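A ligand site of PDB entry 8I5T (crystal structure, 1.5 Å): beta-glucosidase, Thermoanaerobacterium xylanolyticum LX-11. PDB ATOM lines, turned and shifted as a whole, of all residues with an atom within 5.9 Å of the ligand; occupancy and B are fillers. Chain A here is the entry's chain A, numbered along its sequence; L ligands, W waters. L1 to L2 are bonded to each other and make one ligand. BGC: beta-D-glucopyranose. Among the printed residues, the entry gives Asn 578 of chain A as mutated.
Tyr 430 touches the ligand. Thr 435 touches the ligand. CG2 of Val 438 touches O4 of BGC L2 (3.9 Å). Tyr 508 touches the ligand. Trp 510 touches the ligand. CH2 of Trp 516 touches O3 of BGC L2, 3.6 Å away. CH2 of Trp 717 touches C6 of BGC L2, 3.5 Å away. OH of Tyr 775 touches C5 of BGC L2, at 3.7 Å. Hydrophobic or aromatic side chains that line the ligand: Tyr 430, Tyr 432, Val 438, His 492, Tyr 508, Trp 510, Trp 516 and Trp 717. Within 4 Å of the ligand: Glu 426, Tyr 430, Tyr 432, Thr 435, Asp 437, Val 438, His 492, Tyr 508, Trp 510, Trp 516, Thr 576, Asn 578, Trp 717, Glu 762, Arg 771, Tyr 775 and Arg 777.
OE2 of Glu 762 lies within hydrogen-bond range of O6 of BGC L2, 2.6 Å away. OD2 of Asp 437 is in hydrogen-bond range of O3 of BGC L2, 2.7 Å away. A ring nitrogen (NE2) of His 492 sits at hydrogen-bond distance from an oxygen (O3) of BGC L2 (2.8 Å). The backbone carbonyl oxygen (O) of Thr 576 lies within hydrogen-bond range of an oxygen (O4) of BGC L2, at 3.2 Å. O4 of BGC L2 is in hydrogen-bond range of OG1 of Thr 576 (2.8 Å). The guanidinium group (NH1) of Arg 771 is in hydrogen-bond range of an oxygen (O6) of BGC L2, at 2.9 Å. The side-chain hydroxyl (OH) of Tyr 432 lies within hydrogen-bond range of an oxygen (O6) of BGC L1. An oxygen (O4) of BGC L2 is in hydrogen-bond range of the guanidinium group (NH2) of Arg 777. An oxygen (O2) of BGC L2 lies within hydrogen-bond range of the side-chain carboxylate of Glu 426, 2.9 Å away. The side-chain amide nitrogen (ND2) of Asn 578 sits at hydrogen-bond distance from an oxygen (O4) of BGC L1 (3.1 Å).
Water W2 lies within hydrogen-bond range of O3 of BGC L1 (2.7 Å), NE2 of Gln 712 (2.8 Å), OD1 of Asn 578 (3.2 Å) and NH1 of Arg 771 (3.5 Å).
O of Arg 771 is in hydrogen-bond range of N of Glu 762 (3.3 Å). The side-chain carboxylate (OE1) of Glu 762 lies within salt-bridge range of the guanidinium group (NE) of Arg 777 (2.7 Å). The side-chain hydroxyl of Thr 576 sits at hydrogen-bond distance from the side-chain carboxylate of Asp 437. The guanidinium group (NH2) of Arg 771 is in salt-bridge range of the side-chain carboxylate (OE1) of Glu 715, 2.9 Å away. The backbone carbonyl oxygen (O) of Tyr 432 is in hydrogen-bond range of the backbone NH (N) of Glu 426 (2.8 Å). The side-chain carboxylate (OE2) of Glu 426 is in hydrogen-bond range of the side-chain hydroxyl (OH) of Tyr 775, at 2.7 Å. The side-chain carboxylate (OE1) of Glu 426 lies within hydrogen-bond range of the side-chain hydroxyl (OG1) of Thr 435 (2.8 Å). The indole nitrogen (NE1) of Trp 717 sits at hydrogen-bond distance from the side-chain carboxylate (OE1) of Glu 715 (2.9 Å).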
ATOM      1  N   GLU A 426     -24.575 -27.877 -17.165  1.00  0.00           N
ATOM      2  CA  GLU A 426     -23.616 -28.344 -16.152  1.00  0.00           C
ATOM      3  C   GLU A 426     -24.282 -28.243 -14.776  1.00  0.00           C
ATOM      4  O   GLU A 426     -24.291 -29.188 -14.011  1.00  0.00           O
ATOM      5  CB  GLU A 426     -22.333 -27.494 -16.234  1.00  0.00           C
ATOM      6  CG  GLU A 426     -21.272 -27.882 -15.243  1.00  0.00           C
ATOM      7  CD  GLU A 426     -20.017 -27.031 -15.307  1.00  0.00           C
ATOM      8  OE1 GLU A 426     -19.726 -26.431 -16.346  1.00  0.00           O
ATOM      9  OE2 GLU A 426     -19.309 -27.031 -14.271  1.00  0.00           O
ATOM     10  N   ASP A 429     -25.362 -22.756 -11.093  1.00  0.00           N
ATOM     11  CA  ASP A 429     -24.292 -21.847 -10.624  1.00  0.00           C
ATOM     12  C   ASP A 429     -23.265 -21.623 -11.725  1.00  0.00           C
ATOM     13  O   ASP A 429     -22.687 -20.521 -11.841  1.00  0.00           O
ATOM     14  CB  ASP A 429     -23.582 -22.397  -9.404  1.00  0.00           C
ATOM     15  CG  ASP A 429     -24.461 -22.459  -8.177  1.00  0.00           C
ATOM     16  OD1 ASP A 429     -24.757 -21.388  -7.619  1.00  0.00           O
ATOM     17  OD2 ASP A 429     -24.881 -23.569  -7.773  1.00  0.00           O
ATOM     18  N   TYR A 430     -23.012 -22.669 -12.502  1.00  0.00           N
ATOM     19  CA  TYR A 430     -22.092 -22.645 -13.621  1.00  0.00           C
ATOM     20  C   TYR A 430     -22.918 -22.931 -14.880  1.00  0.00           C
ATOM     21  O   TYR A 430     -23.035 -24.089 -15.334  1.00  0.00           O
ATOM     22  CB  TYR A 430     -20.940 -23.658 -13.466  1.00  0.00           C
ATOM     23  CG  TYR A 430     -20.350 -23.846 -12.083  1.00  0.00           C
ATOM     24  CD1 TYR A 430     -20.163 -22.787 -11.193  1.00  0.00           C
ATOM     25  CD2 TYR A 430     -19.920 -25.106 -11.684  1.00  0.00           C
ATOM     26  CE1 TYR A 430     -19.596 -22.990  -9.944  1.00  0.00           C
ATOM     27  CE2 TYR A 430     -19.354 -25.333 -10.435  1.00  0.00           C
ATOM     28  CZ  TYR A 430     -19.181 -24.257  -9.573  1.00  0.00           C
ATOM     29  OH  TYR A 430     -18.628 -24.466  -8.336  1.00  0.00           O
ATOM     30  N   TYR A 432     -23.637 -23.394 -18.057  1.00  0.00           N
ATOM     31  CA  TYR A 432     -23.064 -23.739 -19.355  1.00  0.00           C
ATOM     32  C   TYR A 432     -23.723 -24.996 -19.879  1.00  0.00           C
ATOM     33  O   TYR A 432     -23.860 -25.969 -19.126  1.00  0.00           O
ATOM     34  CB  TYR A 432     -21.573 -24.021 -19.199  1.00  0.00           C
ATOM     35  CG  TYR A 432     -20.841 -22.897 -18.547  1.00  0.00           C
ATOM     36  CD1 TYR A 432     -20.819 -21.639 -19.128  1.00  0.00           C
ATOM     37  CD2 TYR A 432     -20.181 -23.081 -17.338  1.00  0.00           C
ATOM     38  CE1 TYR A 432     -20.160 -20.585 -18.512  1.00  0.00           C
ATOM     39  CE2 TYR A 432     -19.530 -22.056 -16.712  1.00  0.00           C
ATOM     40  CZ  TYR A 432     -19.503 -20.827 -17.300  1.00  0.00           C
ATOM     41  OH  TYR A 432     -18.817 -19.816 -16.639  1.00  0.00           O
ATOM     42  N   THR A 435     -21.338 -29.005 -20.867  1.00  0.00           N
ATOM     43  CA  THR A 435     -19.941 -28.983 -20.510  1.00  0.00           C
ATOM     44  C   THR A 435     -19.278 -30.337 -20.733  1.00  0.00           C
ATOM     45  O   THR A 435     -19.635 -31.302 -20.088  1.00  0.00           O
ATOM     46  CB  THR A 435     -19.751 -28.520 -19.086  1.00  0.00           C
ATOM     47  OG1 THR A 435     -20.281 -27.179 -18.985  1.00  0.00           O
ATOM     48  CG2 THR A 435     -18.284 -28.535 -18.690  1.00  0.00           C
ATOM     49  N   ASP A 437     -16.262 -31.859 -20.421  1.00  0.00           N
ATOM     50  CA  ASP A 437     -15.474 -32.552 -19.397  1.00  0.00           C
ATOM     51  C   ASP A 437     -16.338 -33.154 -18.298  1.00  0.00           C
ATOM     52  O   ASP A 437     -15.908 -34.088 -17.622  1.00  0.00           O
ATOM     53  CB  ASP A 437     -14.416 -31.631 -18.800  1.00  0.00           C
ATOM     54  CG  ASP A 437     -14.980 -30.314 -18.319  1.00  0.00           C
ATOM     55  OD1 ASP A 437     -15.379 -29.478 -19.160  1.00  0.00           O
ATOM     56  OD2 ASP A 437     -14.943 -30.107 -17.128  1.00  0.00           O
ATOM     57  N   VAL A 438     -17.533 -32.600 -18.134  1.00  0.00           N
ATOM     58  CA  VAL A 438     -18.542 -33.081 -17.186  1.00  0.00           C
ATOM     59  C   VAL A 438     -19.449 -34.137 -17.835  1.00  0.00           C
ATOM     60  O   VAL A 438     -19.737 -35.162 -17.186  1.00  0.00           O
ATOM     61  CB  VAL A 438     -19.379 -31.911 -16.633  1.00  0.00           C
ATOM     62  CG1 VAL A 438     -20.437 -32.388 -15.644  1.00  0.00           C
ATOM     63  CG2 VAL A 438     -18.474 -30.906 -15.933  1.00  0.00           C
ATOM     64  N   HIS A 492     -15.188 -26.222 -24.377  1.00  0.00           N
ATOM     65  CA  HIS A 492     -15.650 -26.540 -23.027  1.00  0.00           C
ATOM     66  C   HIS A 492     -17.165 -26.752 -22.951  1.00  0.00           C
ATOM     67  O   HIS A 492     -17.639 -27.646 -22.222  1.00  0.00           O
ATOM     68  CB  HIS A 492     -15.283 -25.405 -22.084  1.00  0.00           C
ATOM     69  CG  HIS A 492     -15.747 -25.582 -20.683  1.00  0.00           C
ATOM     70  ND1 HIS A 492     -16.942 -25.062 -20.226  1.00  0.00           N
ATOM     71  CD2 HIS A 492     -15.160 -26.168 -19.615  1.00  0.00           C
ATOM     72  CE1 HIS A 492     -17.062 -25.310 -18.934  1.00  0.00           C
ATOM     73  NE2 HIS A 492     -15.995 -25.985 -18.541  1.00  0.00           N
ATOM     74  N   TYR A 508     -17.892 -20.388 -21.049  1.00  0.00           N
ATOM     75  CA  TYR A 508     -16.988 -20.464 -19.918  1.00  0.00           C
ATOM     76  C   TYR A 508     -15.762 -19.606 -20.191  1.00  0.00           C
ATOM     77  O   TYR A 508     -15.083 -19.810 -21.195  1.00  0.00           O
ATOM     78  CB  TYR A 508     -16.574 -21.918 -19.704  1.00  0.00           C
ATOM     79  CG  TYR A 508     -15.537 -22.209 -18.640  1.00  0.00           C
ATOM     80  CD1 TYR A 508     -15.880 -22.360 -17.303  1.00  0.00           C
ATOM     81  CD2 TYR A 508     -14.219 -22.467 -19.003  1.00  0.00           C
ATOM     82  CE1 TYR A 508     -14.924 -22.706 -16.344  1.00  0.00           C
ATOM     83  CE2 TYR A 508     -13.271 -22.832 -18.073  1.00  0.00           C
ATOM     84  CZ  TYR A 508     -13.619 -22.930 -16.746  1.00  0.00           C
ATOM     85  OH  TYR A 508     -12.678 -23.292 -15.793  1.00  0.00           O
ATOM     86  N   ASP A 509     -15.516 -18.677 -19.276  1.00  0.00           N
ATOM     87  CA  ASP A 509     -14.358 -17.756 -19.384  1.00  0.00           C
ATOM     88  C   ASP A 509     -13.483 -17.685 -18.122  1.00  0.00           C
ATOM     89  O   ASP A 509     -12.580 -16.826 -18.046  1.00  0.00           O
ATOM     90  CB  ASP A 509     -14.853 -16.355 -19.790  1.00  0.00           C
ATOM     91  CG  ASP A 509     -15.778 -15.713 -18.769  1.00  0.00           C
ATOM     92  OD1 ASP A 509     -16.068 -16.290 -17.713  1.00  0.00           O
ATOM     93  OD2 ASP A 509     -16.239 -14.571 -19.023  1.00  0.00           O
ATOM     94  N   TRP A 510     -13.735 -18.542 -17.144  1.00  0.00           N
ATOM     95  CA  TRP A 510     -12.962 -18.548 -15.895  1.00  0.00           C
ATOM     96  C   TRP A 510     -11.507 -18.952 -16.183  1.00  0.00           C
ATOM     97  O   TRP A 510     -10.577 -18.420 -15.546  1.00  0.00           O
ATOM     98  CB  TRP A 510     -13.598 -19.483 -14.872  1.00  0.00           C
ATOM     99  CG  TRP A 510     -12.932 -19.509 -13.513  1.00  0.00           C
ATOM    100  CD1 TRP A 510     -12.352 -20.593 -12.912  1.00  0.00           C
ATOM    101  CD2 TRP A 510     -12.778 -18.405 -12.610  1.00  0.00           C
ATOM    102  NE1 TRP A 510     -11.856 -20.232 -11.684  1.00  0.00           N
ATOM    103  CE2 TRP A 510     -12.102 -18.898 -11.470  1.00  0.00           C
ATOM    104  CE3 TRP A 510     -13.153 -17.065 -12.632  1.00  0.00           C
ATOM    105  CZ2 TRP A 510     -11.775 -18.093 -10.375  1.00  0.00           C
ATOM    106  CZ3 TRP A 510     -12.825 -16.244 -11.531  1.00  0.00           C
ATOM    107  CH2 TRP A 510     -12.150 -16.769 -10.420  1.00  0.00           C
ATOM    108  N   TRP A 516      -6.826 -26.986 -22.630  1.00  0.00           N
ATOM    109  CA  TRP A 516      -7.075 -28.142 -21.778  1.00  0.00           C
ATOM    110  C   TRP A 516      -6.590 -29.420 -22.478  1.00  0.00           C
ATOM    111  O   TRP A 516      -6.609 -29.512 -23.711  1.00  0.00           O
ATOM    112  CB  TRP A 516      -8.541 -28.236 -21.357  1.00  0.00           C
ATOM    113  CG  TRP A 516      -8.958 -27.280 -20.288  1.00  0.00           C
ATOM    114  CD1 TRP A 516      -8.339 -26.100 -19.957  1.00  0.00           C
ATOM    115  CD2 TRP A 516     -10.095 -27.385 -19.431  1.00  0.00           C
ATOM    116  NE1 TRP A 516      -9.023 -25.475 -18.950  1.00  0.00           N
ATOM    117  CE2 TRP A 516     -10.104 -26.244 -18.606  1.00  0.00           C
ATOM    118  CE3 TRP A 516     -11.106 -28.342 -19.261  1.00  0.00           C
ATOM    119  CZ2 TRP A 516     -11.086 -26.023 -17.628  1.00  0.00           C
ATOM    120  CZ3 TRP A 516     -12.075 -28.122 -18.301  1.00  0.00           C
ATOM    121  CH2 TRP A 516     -12.062 -26.976 -17.505  1.00  0.00           C
ATOM    122  N   THR A 576     -10.381 -30.923 -16.159  1.00  0.00           N
ATOM    123  CA  THR A 576     -11.638 -30.808 -15.391  1.00  0.00           C
ATOM    124  C   THR A 576     -11.417 -30.466 -13.913  1.00  0.00           C
ATOM    125  O   THR A 576     -12.243 -29.764 -13.324  1.00  0.00           O
ATOM    126  CB  THR A 576     -12.543 -32.089 -15.545  1.00  0.00           C
ATOM    127  OG1 THR A 576     -13.923 -31.775 -15.226  1.00  0.00           O
ATOM    128  CG2 THR A 576     -12.104 -33.211 -14.644  1.00  0.00           C
ATOM    129  N   TYR A 577     -10.320 -30.940 -13.323  1.00  0.00           N
ATOM    130  CA  TYR A 577     -10.007 -30.586 -11.932  1.00  0.00           C
ATOM    131  C   TYR A 577      -9.363 -29.233 -12.045  1.00  0.00           C
ATOM    132  O   TYR A 577      -8.162 -29.104 -11.973  1.00  0.00           O
ATOM    133  CB  TYR A 577      -9.086 -31.636 -11.280  1.00  0.00           C
ATOM    134  CG  TYR A 577      -9.772 -32.980 -11.137  1.00  0.00           C
ATOM    135  CD1 TYR A 577      -9.771 -33.902 -12.174  1.00  0.00           C
ATOM    136  CD2 TYR A 577     -10.448 -33.301  -9.966  1.00  0.00           C
ATOM    137  CE1 TYR A 577     -10.431 -35.136 -12.044  1.00  0.00           C
ATOM    138  CE2 TYR A 577     -11.107 -34.512  -9.818  1.00  0.00           C
ATOM    139  CZ  TYR A 577     -11.092 -35.425 -10.860  1.00  0.00           C
ATOM    140  OH  TYR A 577     -11.723 -36.621 -10.707  1.00  0.00           O
ATOM    141  N   ASN A 578     -10.211 -28.219 -12.203  1.00  0.00           N
ATOM    142  CA  ASN A 578      -9.762 -26.914 -12.709  1.00  0.00           C
ATOM    143  C   ASN A 578      -9.111 -25.960 -11.681  1.00  0.00           C
ATOM    144  O   ASN A 578      -8.887 -24.804 -12.007  1.00  0.00           O
ATOM    145  CB  ASN A 578     -10.854 -26.228 -13.541  1.00  0.00           C
ATOM    146  CG  ASN A 578     -12.055 -25.757 -12.721  1.00  0.00           C
ATOM    147  OD1 ASN A 578     -12.237 -26.138 -11.542  1.00  0.00           O
ATOM    148  ND2 ASN A 578     -12.905 -24.911 -13.351  1.00  0.00           N
ATOM    149  N   THR A 579      -8.782 -26.454 -10.487  1.00  0.00           N
ATOM    150  CA  THR A 579      -7.789 -25.801  -9.609  1.00  0.00           C
ATOM    151  C   THR A 579      -6.674 -26.744  -9.076  1.00  0.00           C
ATOM    152  O   THR A 579      -5.782 -26.299  -8.355  1.00  0.00           O
ATOM    153  CB  THR A 579      -8.454 -25.060  -8.442  1.00  0.00           C
ATOM    154  OG1 THR A 579      -9.260 -25.955  -7.677  1.00  0.00           O
ATOM    155  CG2 THR A 579      -9.320 -23.898  -8.958  1.00  0.00           C
ATOM    156  N   GLN A 712      -9.923 -29.001  -4.276  1.00  0.00           N
ATOM    157  CA  GLN A 712     -10.501 -30.109  -5.062  1.00  0.00           C
ATOM    158  C   GLN A 712      -9.997 -31.483  -4.649  1.00  0.00           C
ATOM    159  O   GLN A 712     -10.734 -32.454  -4.724  1.00  0.00           O
ATOM    160  CB  GLN A 712     -10.291 -29.895  -6.546  1.00  0.00           C
ATOM    161  CG  GLN A 712     -11.121 -28.740  -7.033  1.00  0.00           C
ATOM    162  CD  GLN A 712     -10.953 -28.492  -8.505  1.00  0.00           C
ATOM    163  OE1 GLN A 712      -9.967 -28.908  -9.125  1.00  0.00           O
ATOM    164  NE2 GLN A 712     -11.936 -27.798  -9.082  1.00  0.00           N
ATOM    165  N   GLU A 715     -12.118 -32.728  -1.768  1.00  0.00           N
ATOM    166  CA  GLU A 715     -13.527 -32.902  -2.066  1.00  0.00           C
ATOM    167  C   GLU A 715     -13.753 -34.324  -2.547  1.00  0.00           C
ATOM    168  O   GLU A 715     -12.909 -34.909  -3.213  1.00  0.00           O
ATOM    169  CB  GLU A 715     -13.974 -31.952  -3.175  1.00  0.00           C
ATOM    170  CG  GLU A 715     -14.101 -30.498  -2.773  1.00  0.00           C
ATOM    171  CD  GLU A 715     -14.541 -29.569  -3.894  1.00  0.00           C
ATOM    172  OE1 GLU A 715     -14.132 -29.765  -5.064  1.00  0.00           O
ATOM    173  OE2 GLU A 715     -15.288 -28.590  -3.591  1.00  0.00           O
ATOM    174  N   TRP A 717     -16.159 -35.896  -5.256  1.00  0.00           N
ATOM    175  CA  TRP A 717     -16.995 -35.527  -6.411  1.00  0.00           C
ATOM    176  C   TRP A 717     -17.959 -36.677  -6.624  1.00  0.00           C
ATOM    177  O   TRP A 717     -17.543 -37.808  -6.885  1.00  0.00           O
ATOM    178  CB  TRP A 717     -16.151 -35.242  -7.666  1.00  0.00           C
ATOM    179  CG  TRP A 717     -15.428 -33.894  -7.601  1.00  0.00           C
ATOM    180  CD1 TRP A 717     -15.201 -33.126  -6.496  1.00  0.00           C
ATOM    181  CD2 TRP A 717     -14.830 -33.201  -8.701  1.00  0.00           C
ATOM    182  NE1 TRP A 717     -14.489 -31.993  -6.831  1.00  0.00           N
ATOM    183  CE2 TRP A 717     -14.279 -32.000  -8.178  1.00  0.00           C
ATOM    184  CE3 TRP A 717     -14.721 -33.453 -10.062  1.00  0.00           C
ATOM    185  CZ2 TRP A 717     -13.592 -31.071  -8.988  1.00  0.00           C
ATOM    186  CZ3 TRP A 717     -14.048 -32.531 -10.866  1.00  0.00           C
ATOM    187  CH2 TRP A 717     -13.520 -31.351 -10.321  1.00  0.00           C
ATOM    188  N   GLU A 762     -22.106 -31.254  -7.196  1.00  0.00           N
ATOM    189  CA  GLU A 762     -20.796 -31.696  -7.675  1.00  0.00           C
ATOM    190  C   GLU A 762     -20.013 -32.356  -6.546  1.00  0.00           C
ATOM    191  O   GLU A 762     -19.510 -33.469  -6.703  1.00  0.00           O
ATOM    192  CB  GLU A 762     -19.991 -30.506  -8.211  1.00  0.00           C
ATOM    193  CG  GLU A 762     -18.500 -30.726  -8.434  1.00  0.00           C
ATOM    194  CD  GLU A 762     -18.150 -31.331  -9.774  1.00  0.00           C
ATOM    195  OE1 GLU A 762     -18.500 -32.507 -10.032  1.00  0.00           O
ATOM    196  OE2 GLU A 762     -17.500 -30.645 -10.592  1.00  0.00           O
ATOM    197  N   ARG A 771     -20.554 -28.003  -2.796  1.00  0.00           N
ATOM    198  CA  ARG A 771     -20.342 -27.060  -3.862  1.00  0.00           C
ATOM    199  C   ARG A 771     -21.159 -27.486  -5.080  1.00  0.00           C
ATOM    200  O   ARG A 771     -21.056 -28.640  -5.518  1.00  0.00           O
ATOM    201  CB  ARG A 771     -18.855 -26.972  -4.220  1.00  0.00           C
ATOM    202  CG  ARG A 771     -18.523 -26.003  -5.333  1.00  0.00           C
ATOM    203  CD  ARG A 771     -17.023 -25.814  -5.444  1.00  0.00           C
ATOM    204  NE  ARG A 771     -16.321 -27.028  -5.854  1.00  0.00           N
ATOM    205  CZ  ARG A 771     -16.226 -27.468  -7.100  1.00  0.00           C
ATOM    206  NH1 ARG A 771     -16.811 -26.836  -8.097  1.00  0.00           N
ATOM    207  NH2 ARG A 771     -15.519 -28.581  -7.355  1.00  0.00           N
ATOM    208  N   TYR A 775     -26.303 -30.741 -10.118  1.00  0.00           N
ATOM    209  CA  TYR A 775     -25.125 -30.872 -10.932  1.00  0.00           C
ATOM    210  C   TYR A 775     -25.239 -32.057 -11.885  1.00  0.00           C
ATOM    211  O   TYR A 775     -25.813 -33.086 -11.530  1.00  0.00           O
ATOM    212  CB  TYR A 775     -23.879 -31.014 -10.049  1.00  0.00           C
ATOM    213  CG  TYR A 775     -22.614 -30.558 -10.768  1.00  0.00           C
ATOM    214  CD1 TYR A 775     -22.353 -29.205 -10.955  1.00  0.00           C
ATOM    215  CD2 TYR A 775     -21.690 -31.475 -11.278  1.00  0.00           C
ATOM    216  CE1 TYR A 775     -21.217 -28.779 -11.634  1.00  0.00           C
ATOM    217  CE2 TYR A 775     -20.561 -31.052 -11.981  1.00  0.00           C
ATOM    218  CZ  TYR A 775     -20.335 -29.701 -12.156  1.00  0.00           C
ATOM    219  OH  TYR A 775     -19.220 -29.278 -12.841  1.00  0.00           O
ATOM    220  N   ARG A 777     -22.868 -34.073 -13.284  1.00  0.00           N
ATOM    221  CA  ARG A 777     -21.911 -35.188 -13.166  1.00  0.00           C
ATOM    222  C   ARG A 777     -22.436 -36.475 -12.490  1.00  0.00           C
ATOM    223  O   ARG A 777     -22.133 -37.552 -13.003  1.00  0.00           O
ATOM    224  CB  ARG A 777     -20.595 -34.731 -12.534  1.00  0.00           C
ATOM    225  CG  ARG A 777     -19.359 -35.450 -13.074  1.00  0.00           C
ATOM    226  CD  ARG A 777     -18.041 -35.156 -12.360  1.00  0.00           C
ATOM    227  NE  ARG A 777     -17.684 -33.736 -12.314  1.00  0.00           N
ATOM    228  CZ  ARG A 777     -16.922 -33.077 -13.185  1.00  0.00           C
ATOM    229  NH1 ARG A 777     -16.371 -33.666 -14.254  1.00  0.00           N
ATOM    230  NH2 ARG A 777     -16.654 -31.790 -12.964  1.00  0.00           N
HETATM  231  C2  BGC L   1     -15.648 -22.458  -9.850  1.00  0.00           C
HETATM  232  C3  BGC L   1     -15.464 -23.596 -10.860  1.00  0.00           C
HETATM  233  C4  BGC L   1     -16.386 -23.438 -12.068  1.00  0.00           C
HETATM  234  C5  BGC L   1     -16.394 -22.022 -12.609  1.00  0.00           C
HETATM  235  C6  BGC L   1     -17.469 -21.815 -13.659  1.00  0.00           C
HETATM  236  C1  BGC L   1     -15.597 -21.131 -10.579  1.00  0.00           C
HETATM  237  O1  BGC L   1     -15.891 -20.063  -9.680  1.00  0.00           O
HETATM  238  O2  BGC L   1     -14.613 -22.579  -8.872  1.00  0.00           O
HETATM  239  O3  BGC L   1     -15.662 -24.861 -10.226  1.00  0.00           O
HETATM  240  O4  BGC L   1     -15.927 -24.211 -13.166  1.00  0.00           O
HETATM  241  O5  BGC L   1     -16.636 -21.117 -11.554  1.00  0.00           O
HETATM  242  O6  BGC L   1     -17.243 -20.550 -14.328  1.00  0.00           O
HETATM  243  C2  BGC L   2     -16.143 -25.897 -14.811  1.00  0.00           C
HETATM  244  C3  BGC L   2     -16.038 -27.392 -15.094  1.00  0.00           C
HETATM  245  C4  BGC L   2     -15.264 -28.112 -14.002  1.00  0.00           C
HETATM  246  C5  BGC L   2     -15.872 -27.780 -12.635  1.00  0.00           C
HETATM  247  C6  BGC L   2     -15.184 -28.498 -11.491  1.00  0.00           C
HETATM  248  C1  BGC L   2     -16.438 -25.539 -13.353  1.00  0.00           C
HETATM  249  O2  BGC L   2     -17.110 -25.288 -15.680  1.00  0.00           O
HETATM  250  O3  BGC L   2     -15.416 -27.576 -16.363  1.00  0.00           O
HETATM  251  O4  BGC L   2     -15.270 -29.546 -14.235  1.00  0.00           O
HETATM  252  O5  BGC L   2     -15.762 -26.369 -12.414  1.00  0.00           O
HETATM  253  O6  BGC L   2     -16.031 -28.477 -10.336  1.00  0.00           O
HETATM  254  O   HOH W   1     -18.894 -19.328 -11.059  1.00  0.00           O
HETATM  255  O   HOH W   2     -13.607 -25.631  -8.710  1.00  0.00           O
HETATM  256  O   HOH W   3     -17.008 -18.059 -13.187  1.00  0.00           O
HETATM  257  O   HOH W   4     -15.288 -22.754  -6.222  1.00  0.00           O
